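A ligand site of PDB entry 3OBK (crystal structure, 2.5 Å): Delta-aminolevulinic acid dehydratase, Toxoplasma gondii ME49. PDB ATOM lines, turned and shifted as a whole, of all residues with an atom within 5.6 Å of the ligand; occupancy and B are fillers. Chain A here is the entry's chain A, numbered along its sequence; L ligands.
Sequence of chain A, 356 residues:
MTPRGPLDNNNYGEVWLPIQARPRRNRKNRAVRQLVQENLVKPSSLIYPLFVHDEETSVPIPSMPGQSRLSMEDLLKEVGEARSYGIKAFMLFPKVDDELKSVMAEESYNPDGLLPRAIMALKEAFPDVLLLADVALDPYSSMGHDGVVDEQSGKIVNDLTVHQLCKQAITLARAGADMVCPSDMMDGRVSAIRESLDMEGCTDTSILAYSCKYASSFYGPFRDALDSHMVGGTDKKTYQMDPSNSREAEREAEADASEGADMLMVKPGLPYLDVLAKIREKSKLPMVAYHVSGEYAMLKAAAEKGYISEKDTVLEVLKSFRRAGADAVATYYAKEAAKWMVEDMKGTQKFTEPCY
OG of Ser 183 sits at hydrogen-bond distance from N2 of the ligand. The guanidinium group (NH2) of Arg 223 lies within salt-bridge range of an oxygen (O2) of the ligand, 2.6 Å away. The side-chain hydroxyl of Tyr 332 sits at hydrogen-bond distance from an oxygen (O3) of the ligand. The backbone NH (N) of Ser 293 is in hydrogen-bond range of an oxygen (O3) of the ligand (2.9 Å). The side-chain hydroxyl (OG) of Ser 293 lies within hydrogen-bond range of an oxygen (O4) of the ligand. The side-chain amino group of Lys 213 is in salt-bridge range of an oxygen (O1) of the ligand. The side-chain carboxylate of Asp 138 is in salt-bridge range of a nitrogen (N2) of the ligand. An oxygen (O2) of the ligand is in salt-bridge range of the side-chain amino group of Lys 236. OD2 of Asp 146 is in salt-bridge range of N2 of the ligand, at 3.0 Å. The side-chain amide nitrogen of Gln 240 lies within hydrogen-bond range of an oxygen (O1) of the ligand, 3.1 Å away. The side-chain carboxylate (OD1) of Asp 134 is in hydrogen-bond range of a nitrogen (N1) of the ligand (3.4 Å).
The backbone carbonyl oxygen (O) of Ser 183 is in hydrogen-bond range of the side-chain amino group (NZ) of Lys 213, 3.0 Å away. OD1 of Asp 134 lies within hydrogen-bond range of OG of Ser 183 (2.8 Å). The backbone NH (N) of Ser 183 is in hydrogen-bond range of the backbone carbonyl oxygen (O) of Val 135 (2.9 Å). The side-chain hydroxyl (OH) of Tyr 332 sits at hydrogen-bond distance from the side-chain hydroxyl (OH) of Tyr 290 (3.0 Å). OG of Ser 293 lies within hydrogen-bond range of N of Phe 222, at 3.0 Å. The side-chain hydroxyl (OG) of Ser 293 lies within hydrogen-bond range of the backbone carbonyl oxygen (O) of Phe 218 (3.4 Å). The side-chain carboxylate of Asp 138 is in salt-bridge range of the side-chain amino group of Lys 236 (3.2 Å). The side-chain amino group of Lys 236 lies within salt-bridge range of the side-chain carboxylate of Asp 146 (2.6 Å).
Residues that only touch the ligand: Lys 267, Phe 222, Ala 136, Val 292, Tyr 219, Tyr 290 and Phe 93. Hydrophobic or aromatic side chains that line the ligand: Phe 93, Ala 136, Tyr 219, Phe 222, Tyr 290, Val 292 and Tyr 332. Of the 26 residues printed, 17 come within 4 Å of the ligand.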
ATOM      1  N   MET A  64       5.632 -11.363  -9.495  1.00  0.00           N
ATOM      2  CA  MET A  64       4.343 -10.670  -9.633  1.00  0.00           C
ATOM      3  C   MET A  64       3.236 -11.520  -8.990  1.00  0.00           C
ATOM      4  O   MET A  64       2.392 -12.077  -9.677  1.00  0.00           O
ATOM      5  CB  MET A  64       4.022 -10.469 -11.096  1.00  0.00           C
ATOM      6  CG  MET A  64       5.081  -9.743 -11.848  1.00  0.00           C
ATOM      7  SD  MET A  64       4.568  -9.391 -13.531  1.00  0.00           S
ATOM      8  CE  MET A  64       3.068  -8.442 -13.287  1.00  0.00           C
ATOM      9  N   PHE A  93       0.457 -10.381 -23.672  1.00  0.00           N
ATOM     10  CA  PHE A  93       1.872 -10.536 -23.858  1.00  0.00           C
ATOM     11  C   PHE A  93       2.185 -12.034 -23.959  1.00  0.00           C
ATOM     12  O   PHE A  93       1.663 -12.821 -23.189  1.00  0.00           O
ATOM     13  CB  PHE A  93       2.591  -9.941 -22.659  1.00  0.00           C
ATOM     14  CG  PHE A  93       2.383  -8.471 -22.481  1.00  0.00           C
ATOM     15  CD1 PHE A  93       3.085  -7.555 -23.237  1.00  0.00           C
ATOM     16  CD2 PHE A  93       1.550  -8.000 -21.493  1.00  0.00           C
ATOM     17  CE1 PHE A  93       2.930  -6.198 -23.032  1.00  0.00           C
ATOM     18  CE2 PHE A  93       1.403  -6.664 -21.258  1.00  0.00           C
ATOM     19  CZ  PHE A  93       2.072  -5.763 -22.017  1.00  0.00           C
ATOM     20  N   ASP A 134       0.754  -5.947 -27.804  1.00  0.00           N
ATOM     21  CA  ASP A 134       1.963  -5.168 -27.815  1.00  0.00           C
ATOM     22  C   ASP A 134       2.651  -5.308 -29.184  1.00  0.00           C
ATOM     23  O   ASP A 134       2.484  -6.324 -29.872  1.00  0.00           O
ATOM     24  CB  ASP A 134       2.867  -5.657 -26.703  1.00  0.00           C
ATOM     25  CG  ASP A 134       4.074  -4.781 -26.494  1.00  0.00           C
ATOM     26  OD1 ASP A 134       4.038  -3.896 -25.591  1.00  0.00           O
ATOM     27  OD2 ASP A 134       5.058  -4.990 -27.241  1.00  0.00           O
ATOM     28  N   VAL A 135       3.388  -4.263 -29.593  1.00  0.00           N
ATOM     29  CA  VAL A 135       4.269  -4.309 -30.761  1.00  0.00           C
ATOM     30  C   VAL A 135       5.675  -3.922 -30.299  1.00  0.00           C
ATOM     31  O   VAL A 135       5.872  -2.873 -29.707  1.00  0.00           O
ATOM     32  CB  VAL A 135       3.782  -3.422 -31.915  1.00  0.00           C
ATOM     33  CG1 VAL A 135       4.837  -3.334 -33.037  1.00  0.00           C
ATOM     34  CG2 VAL A 135       2.430  -3.925 -32.434  1.00  0.00           C
ATOM     35  N   ALA A 136       6.614  -4.805 -30.560  1.00  0.00           N
ATOM     36  CA  ALA A 136       7.964  -4.726 -30.006  1.00  0.00           C
ATOM     37  C   ALA A 136       8.561  -6.109 -30.124  1.00  0.00           C
ATOM     38  O   ALA A 136       7.859  -7.123 -30.055  1.00  0.00           O
ATOM     39  CB  ALA A 136       7.971  -4.267 -28.549  1.00  0.00           C
ATOM     40  N   ASP A 138      10.956  -7.456 -28.247  1.00  0.00           N
ATOM     41  CA  ASP A 138      11.719  -8.034 -27.137  1.00  0.00           C
ATOM     42  C   ASP A 138      11.223  -9.388 -26.687  1.00  0.00           C
ATOM     43  O   ASP A 138      12.016 -10.187 -26.250  1.00  0.00           O
ATOM     44  CB  ASP A 138      11.975  -7.098 -25.939  1.00  0.00           C
ATOM     45  CG  ASP A 138      10.801  -6.246 -25.550  1.00  0.00           C
ATOM     46  OD1 ASP A 138      10.085  -5.695 -26.418  1.00  0.00           O
ATOM     47  OD2 ASP A 138      10.670  -6.046 -24.331  1.00  0.00           O
ATOM     48  N   PRO A 139       9.923  -9.663 -26.804  1.00  0.00           N
ATOM     49  CA  PRO A 139       9.516 -10.994 -26.388  1.00  0.00           C
ATOM     50  C   PRO A 139      10.033 -12.071 -27.317  1.00  0.00           C
ATOM     51  O   PRO A 139       9.993 -13.247 -26.988  1.00  0.00           O
ATOM     52  CB  PRO A 139       7.969 -10.952 -26.432  1.00  0.00           C
ATOM     53  CG  PRO A 139       7.593  -9.486 -26.441  1.00  0.00           C
ATOM     54  CD  PRO A 139       8.773  -8.755 -27.034  1.00  0.00           C
ATOM     55  N   ASP A 146      13.969  -4.449 -27.825  1.00  0.00           N
ATOM     56  CA  ASP A 146      12.740  -4.156 -28.551  1.00  0.00           C
ATOM     57  C   ASP A 146      12.977  -4.010 -30.041  1.00  0.00           C
ATOM     58  O   ASP A 146      12.036  -3.953 -30.817  1.00  0.00           O
ATOM     59  CB  ASP A 146      12.093  -2.868 -28.045  1.00  0.00           C
ATOM     60  CG  ASP A 146      11.721  -2.912 -26.566  1.00  0.00           C
ATOM     61  OD1 ASP A 146      12.409  -3.570 -25.762  1.00  0.00           O
ATOM     62  OD2 ASP A 146      10.765  -2.213 -26.193  1.00  0.00           O
ATOM     63  N   SER A 183       5.402  -0.476 -28.138  1.00  0.00           N
ATOM     64  CA  SER A 183       6.129  -0.105 -26.917  1.00  0.00           C
ATOM     65  C   SER A 183       7.634  -0.029 -27.147  1.00  0.00           C
ATOM     66  O   SER A 183       8.414  -0.011 -26.189  1.00  0.00           O
ATOM     67  CB  SER A 183       5.852  -1.132 -25.840  1.00  0.00           C
ATOM     68  OG  SER A 183       6.309  -2.398 -26.263  1.00  0.00           O
ATOM     69  N   ASP A 184       8.024   0.094 -28.412  1.00  0.00           N
ATOM     70  CA  ASP A 184       9.400  -0.086 -28.853  1.00  0.00           C
ATOM     71  C   ASP A 184      10.298   1.111 -28.691  1.00  0.00           C
ATOM     72  O   ASP A 184      11.498   0.943 -28.546  1.00  0.00           O
ATOM     73  CB  ASP A 184       9.387  -0.409 -30.349  1.00  0.00           C
ATOM     74  CG  ASP A 184       8.532   0.576 -31.133  1.00  0.00           C
ATOM     75  OD1 ASP A 184       7.296   0.510 -30.981  1.00  0.00           O
ATOM     76  OD2 ASP A 184       9.111   1.430 -31.854  1.00  0.00           O
ATOM     77  N   TYR A 210       2.872   4.266 -27.236  1.00  0.00           N
ATOM     78  CA  TYR A 210       3.663   4.540 -26.031  1.00  0.00           C
ATOM     79  C   TYR A 210       4.560   5.714 -26.396  1.00  0.00           C
ATOM     80  O   TYR A 210       5.584   5.506 -26.984  1.00  0.00           O
ATOM     81  CB  TYR A 210       4.503   3.354 -25.641  1.00  0.00           C
ATOM     82  CG  TYR A 210       3.793   2.188 -25.036  1.00  0.00           C
ATOM     83  CD1 TYR A 210       3.078   1.314 -25.798  1.00  0.00           C
ATOM     84  CD2 TYR A 210       3.923   1.911 -23.686  1.00  0.00           C
ATOM     85  CE1 TYR A 210       2.445   0.192 -25.232  1.00  0.00           C
ATOM     86  CE2 TYR A 210       3.290   0.806 -23.107  1.00  0.00           C
ATOM     87  CZ  TYR A 210       2.553  -0.056 -23.884  1.00  0.00           C
ATOM     88  OH  TYR A 210       1.935  -1.168 -23.295  1.00  0.00           O
ATOM     89  N   LYS A 213       7.730   6.655 -22.729  1.00  0.00           N
ATOM     90  CA  LYS A 213       8.075   5.423 -22.055  1.00  0.00           C
ATOM     91  C   LYS A 213       9.515   5.556 -21.592  1.00  0.00           C
ATOM     92  O   LYS A 213      10.402   5.781 -22.414  1.00  0.00           O
ATOM     93  CB  LYS A 213       7.965   4.228 -22.992  1.00  0.00           C
ATOM     94  CG  LYS A 213       8.515   2.983 -22.377  1.00  0.00           C
ATOM     95  CD  LYS A 213       8.177   1.771 -23.206  1.00  0.00           C
ATOM     96  CE  LYS A 213       8.595   0.527 -22.512  1.00  0.00           C
ATOM     97  NZ  LYS A 213       8.147  -0.638 -23.235  1.00  0.00           N
ATOM     98  N   PHE A 218      11.652  -0.285 -13.061  1.00  0.00           N
ATOM     99  CA  PHE A 218      10.451  -0.937 -12.550  1.00  0.00           C
ATOM    100  C   PHE A 218       9.838  -1.992 -13.471  1.00  0.00           C
ATOM    101  O   PHE A 218       8.729  -2.469 -13.189  1.00  0.00           O
ATOM    102  CB  PHE A 218       9.358   0.103 -12.267  1.00  0.00           C
ATOM    103  CG  PHE A 218       9.653   0.960 -11.092  1.00  0.00           C
ATOM    104  CD1 PHE A 218       9.407   0.499  -9.822  1.00  0.00           C
ATOM    105  CD2 PHE A 218      10.157   2.241 -11.259  1.00  0.00           C
ATOM    106  CE1 PHE A 218       9.673   1.284  -8.721  1.00  0.00           C
ATOM    107  CE2 PHE A 218      10.432   3.017 -10.199  1.00  0.00           C
ATOM    108  CZ  PHE A 218      10.198   2.553  -8.911  1.00  0.00           C
ATOM    109  N   TYR A 219      10.514  -2.353 -14.568  1.00  0.00           N
ATOM    110  CA  TYR A 219      10.023  -3.353 -15.509  1.00  0.00           C
ATOM    111  C   TYR A 219      10.514  -4.763 -15.214  1.00  0.00           C
ATOM    112  O   TYR A 219      10.289  -5.691 -16.002  1.00  0.00           O
ATOM    113  CB  TYR A 219      10.473  -3.034 -16.940  1.00  0.00           C
ATOM    114  CG  TYR A 219      10.109  -1.689 -17.496  1.00  0.00           C
ATOM    115  CD1 TYR A 219       8.861  -1.174 -17.348  1.00  0.00           C
ATOM    116  CD2 TYR A 219      11.031  -0.962 -18.220  1.00  0.00           C
ATOM    117  CE1 TYR A 219       8.526   0.040 -17.874  1.00  0.00           C
ATOM    118  CE2 TYR A 219      10.710   0.245 -18.772  1.00  0.00           C
ATOM    119  CZ  TYR A 219       9.455   0.763 -18.592  1.00  0.00           C
ATOM    120  OH  TYR A 219       9.152   1.974 -19.129  1.00  0.00           O
ATOM    121  N   GLY A 220      11.207  -4.942 -14.110  1.00  0.00           N
ATOM    122  CA  GLY A 220      11.908  -6.209 -13.875  1.00  0.00           C
ATOM    123  C   GLY A 220      11.003  -7.428 -13.828  1.00  0.00           C
ATOM    124  O   GLY A 220      11.301  -8.440 -14.477  1.00  0.00           O
ATOM    125  N   PHE A 222       8.024  -7.889 -15.056  1.00  0.00           N
ATOM    126  CA  PHE A 222       7.548  -8.176 -16.408  1.00  0.00           C
ATOM    127  C   PHE A 222       8.604  -9.035 -17.175  1.00  0.00           C
ATOM    128  O   PHE A 222       8.255 -10.045 -17.804  1.00  0.00           O
ATOM    129  CB  PHE A 222       7.230  -6.865 -17.136  1.00  0.00           C
ATOM    130  CG  PHE A 222       6.836  -7.046 -18.601  1.00  0.00           C
ATOM    131  CD1 PHE A 222       7.821  -7.158 -19.583  1.00  0.00           C
ATOM    132  CD2 PHE A 222       5.493  -7.037 -18.975  1.00  0.00           C
ATOM    133  CE1 PHE A 222       7.464  -7.290 -20.908  1.00  0.00           C
ATOM    134  CE2 PHE A 222       5.109  -7.147 -20.298  1.00  0.00           C
ATOM    135  CZ  PHE A 222       6.090  -7.307 -21.275  1.00  0.00           C
ATOM    136  N   ARG A 223       9.876  -8.641 -17.117  1.00  0.00           N
ATOM    137  CA  ARG A 223      10.922  -9.360 -17.816  1.00  0.00           C
ATOM    138  C   ARG A 223      11.161 -10.755 -17.233  1.00  0.00           C
ATOM    139  O   ARG A 223      11.654 -11.633 -17.927  1.00  0.00           O
ATOM    140  CB  ARG A 223      12.199  -8.529 -17.825  1.00  0.00           C
ATOM    141  CG  ARG A 223      12.087  -7.270 -18.686  1.00  0.00           C
ATOM    142  CD  ARG A 223      13.268  -6.359 -18.508  1.00  0.00           C
ATOM    143  NE  ARG A 223      13.126  -5.069 -19.201  1.00  0.00           N
ATOM    144  CZ  ARG A 223      13.878  -3.999 -18.945  1.00  0.00           C
ATOM    145  NH1 ARG A 223      14.823  -4.040 -18.006  1.00  0.00           N
ATOM    146  NH2 ARG A 223      13.684  -2.871 -19.614  1.00  0.00           N
ATOM    147  N   LYS A 236      18.522  -0.278 -22.116  1.00  0.00           N
ATOM    148  CA  LYS A 236      17.670   0.259 -23.167  1.00  0.00           C
ATOM    149  C   LYS A 236      17.712   1.784 -23.236  1.00  0.00           C
ATOM    150  O   LYS A 236      16.818   2.421 -23.751  1.00  0.00           O
ATOM    151  CB  LYS A 236      16.234  -0.246 -23.012  1.00  0.00           C
ATOM    152  CG  LYS A 236      16.094  -1.755 -22.862  1.00  0.00           C
ATOM    153  CD  LYS A 236      14.660  -2.195 -23.030  1.00  0.00           C
ATOM    154  CE  LYS A 236      14.476  -3.712 -23.135  1.00  0.00           C
ATOM    155  NZ  LYS A 236      13.010  -4.095 -23.288  1.00  0.00           N
ATOM    156  N   GLN A 240      14.554   3.904 -24.810  1.00  0.00           N
ATOM    157  CA  GLN A 240      13.682   4.394 -23.749  1.00  0.00           C
ATOM    158  C   GLN A 240      14.257   5.700 -23.197  1.00  0.00           C
ATOM    159  O   GLN A 240      15.449   5.975 -23.311  1.00  0.00           O
ATOM    160  CB  GLN A 240      13.488   3.335 -22.685  1.00  0.00           C
ATOM    161  CG  GLN A 240      12.734   2.084 -23.221  1.00  0.00           C
ATOM    162  CD  GLN A 240      12.666   0.927 -22.226  1.00  0.00           C
ATOM    163  OE1 GLN A 240      13.235   0.979 -21.125  1.00  0.00           O
ATOM    164  NE2 GLN A 240      11.984  -0.146 -22.629  1.00  0.00           N
ATOM    165  N   LYS A 267       4.399   5.667 -19.423  1.00  0.00           N
ATOM    166  CA  LYS A 267       4.796   4.489 -18.704  1.00  0.00           C
ATOM    167  C   LYS A 267       6.207   4.681 -18.289  1.00  0.00           C
ATOM    168  O   LYS A 267       7.010   5.141 -19.091  1.00  0.00           O
ATOM    169  CB  LYS A 267       4.759   3.337 -19.657  1.00  0.00           C
ATOM    170  CG  LYS A 267       5.239   1.974 -19.150  1.00  0.00           C
ATOM    171  CD  LYS A 267       5.025   1.048 -20.305  1.00  0.00           C
ATOM    172  CE  LYS A 267       5.816  -0.210 -20.315  1.00  0.00           C
ATOM    173  NZ  LYS A 267       5.807  -0.711 -21.745  1.00  0.00           N
ATOM    174  N   TYR A 290       0.337   3.308 -17.492  1.00  0.00           N
ATOM    175  CA  TYR A 290       0.618   1.904 -17.196  1.00  0.00           C
ATOM    176  C   TYR A 290       1.181   1.801 -15.778  1.00  0.00           C
ATOM    177  O   TYR A 290       2.278   2.291 -15.481  1.00  0.00           O
ATOM    178  CB  TYR A 290       1.620   1.350 -18.187  1.00  0.00           C
ATOM    179  CG  TYR A 290       1.561  -0.139 -18.416  1.00  0.00           C
ATOM    180  CD1 TYR A 290       1.659  -1.052 -17.374  1.00  0.00           C
ATOM    181  CD2 TYR A 290       1.455  -0.643 -19.705  1.00  0.00           C
ATOM    182  CE1 TYR A 290       1.637  -2.460 -17.630  1.00  0.00           C
ATOM    183  CE2 TYR A 290       1.400  -2.012 -19.960  1.00  0.00           C
ATOM    184  CZ  TYR A 290       1.505  -2.911 -18.936  1.00  0.00           C
ATOM    185  OH  TYR A 290       1.469  -4.244 -19.270  1.00  0.00           O
ATOM    186  N   HIS A 291       0.402   1.144 -14.916  1.00  0.00           N
ATOM    187  CA  HIS A 291       0.820   0.738 -13.586  1.00  0.00           C
ATOM    188  C   HIS A 291       1.623  -0.557 -13.741  1.00  0.00           C
ATOM    189  O   HIS A 291       1.035  -1.653 -13.829  1.00  0.00           O
ATOM    190  CB  HIS A 291      -0.425   0.511 -12.745  1.00  0.00           C
ATOM    191  CG  HIS A 291      -0.169   0.389 -11.280  1.00  0.00           C
ATOM    192  ND1 HIS A 291      -0.843  -0.520 -10.482  1.00  0.00           N
ATOM    193  CD2 HIS A 291       0.666   1.061 -10.448  1.00  0.00           C
ATOM    194  CE1 HIS A 291      -0.428  -0.396  -9.231  1.00  0.00           C
ATOM    195  NE2 HIS A 291       0.482   0.562  -9.184  1.00  0.00           N
ATOM    196  N   VAL A 292       2.955  -0.438 -13.797  1.00  0.00           N
ATOM    197  CA  VAL A 292       3.796  -1.498 -14.310  1.00  0.00           C
ATOM    198  C   VAL A 292       4.140  -2.557 -13.278  1.00  0.00           C
ATOM    199  O   VAL A 292       3.983  -2.357 -12.080  1.00  0.00           O
ATOM    200  CB  VAL A 292       5.110  -0.959 -14.883  1.00  0.00           C
ATOM    201  CG1 VAL A 292       4.850   0.133 -15.896  1.00  0.00           C
ATOM    202  CG2 VAL A 292       6.044  -0.487 -13.770  1.00  0.00           C
ATOM    203  N   SER A 293       4.651  -3.695 -13.777  1.00  0.00           N
ATOM    204  CA  SER A 293       4.917  -4.871 -12.979  1.00  0.00           C
ATOM    205  C   SER A 293       5.643  -4.550 -11.678  1.00  0.00           C
ATOM    206  O   SER A 293       5.317  -5.070 -10.631  1.00  0.00           O
ATOM    207  CB  SER A 293       5.747  -5.835 -13.791  1.00  0.00           C
ATOM    208  OG  SER A 293       7.015  -5.275 -14.122  1.00  0.00           O
ATOM    209  N   GLY A 294       6.622  -3.692 -11.753  1.00  0.00           N
ATOM    210  CA  GLY A 294       7.400  -3.349 -10.571  1.00  0.00           C
ATOM    211  C   GLY A 294       6.569  -2.622  -9.536  1.00  0.00           C
ATOM    212  O   GLY A 294       6.705  -2.872  -8.349  1.00  0.00           O
ATOM    213  N   TYR A 332      -2.225  -4.501 -13.424  1.00  0.00           N
ATOM    214  CA  TYR A 332      -2.370  -5.919 -13.076  1.00  0.00           C
ATOM    215  C   TYR A 332      -3.395  -6.094 -11.950  1.00  0.00           C
ATOM    216  O   TYR A 332      -3.877  -7.209 -11.720  1.00  0.00           O
ATOM    217  CB  TYR A 332      -0.998  -6.540 -12.747  1.00  0.00           C
ATOM    218  CG  TYR A 332      -0.036  -6.417 -13.898  1.00  0.00           C
ATOM    219  CD1 TYR A 332      -0.123  -7.240 -15.002  1.00  0.00           C
ATOM    220  CD2 TYR A 332       0.925  -5.415 -13.910  1.00  0.00           C
ATOM    221  CE1 TYR A 332       0.730  -7.110 -16.046  1.00  0.00           C
ATOM    222  CE2 TYR A 332       1.796  -5.263 -14.962  1.00  0.00           C
ATOM    223  CZ  TYR A 332       1.699  -6.112 -16.053  1.00  0.00           C
ATOM    224  OH  TYR A 332       2.558  -5.957 -17.123  1.00  0.00           O
HETATM  225  C1  LIG L   1       8.247  -4.509 -24.088  1.00  0.00           C
HETATM  226  C2  LIG L   1       7.432  -4.232 -22.872  1.00  0.00           C
HETATM  227  C3  LIG L   1       7.919  -4.043 -21.578  1.00  0.00           C
HETATM  228  C4  LIG L   1       6.811  -3.811 -20.787  1.00  0.00           C
HETATM  229  C5  LIG L   1       5.706  -3.765 -21.622  1.00  0.00           C
HETATM  230  N1  LIG L   1       6.107  -4.045 -22.874  1.00  0.00           N
HETATM  231  C6  LIG L   1       9.324  -4.247 -21.060  1.00  0.00           C
HETATM  232  C7  LIG L   1      10.344  -3.278 -21.500  1.00  0.00           C
HETATM  233  O1  LIG L   1      10.066  -2.602 -22.525  1.00  0.00           O
HETATM  234  O2  LIG L   1      11.439  -3.210 -20.912  1.00  0.00           O
HETATM  235  C8  LIG L   1       6.829  -3.636 -19.318  1.00  0.00           C
HETATM  236  C9  LIG L   1       5.527  -3.685 -18.621  1.00  0.00           C
HETATM  237  C10 LIG L   1       5.525  -3.813 -17.151  1.00  0.00           C
HETATM  238  O3  LIG L   1       4.511  -4.275 -16.626  1.00  0.00           O
HETATM  239  O4  LIG L   1       6.550  -3.770 -16.460  1.00  0.00           O
HETATM  240  N2  LIG L   1       8.284  -3.526 -25.118  1.00  0.00           N
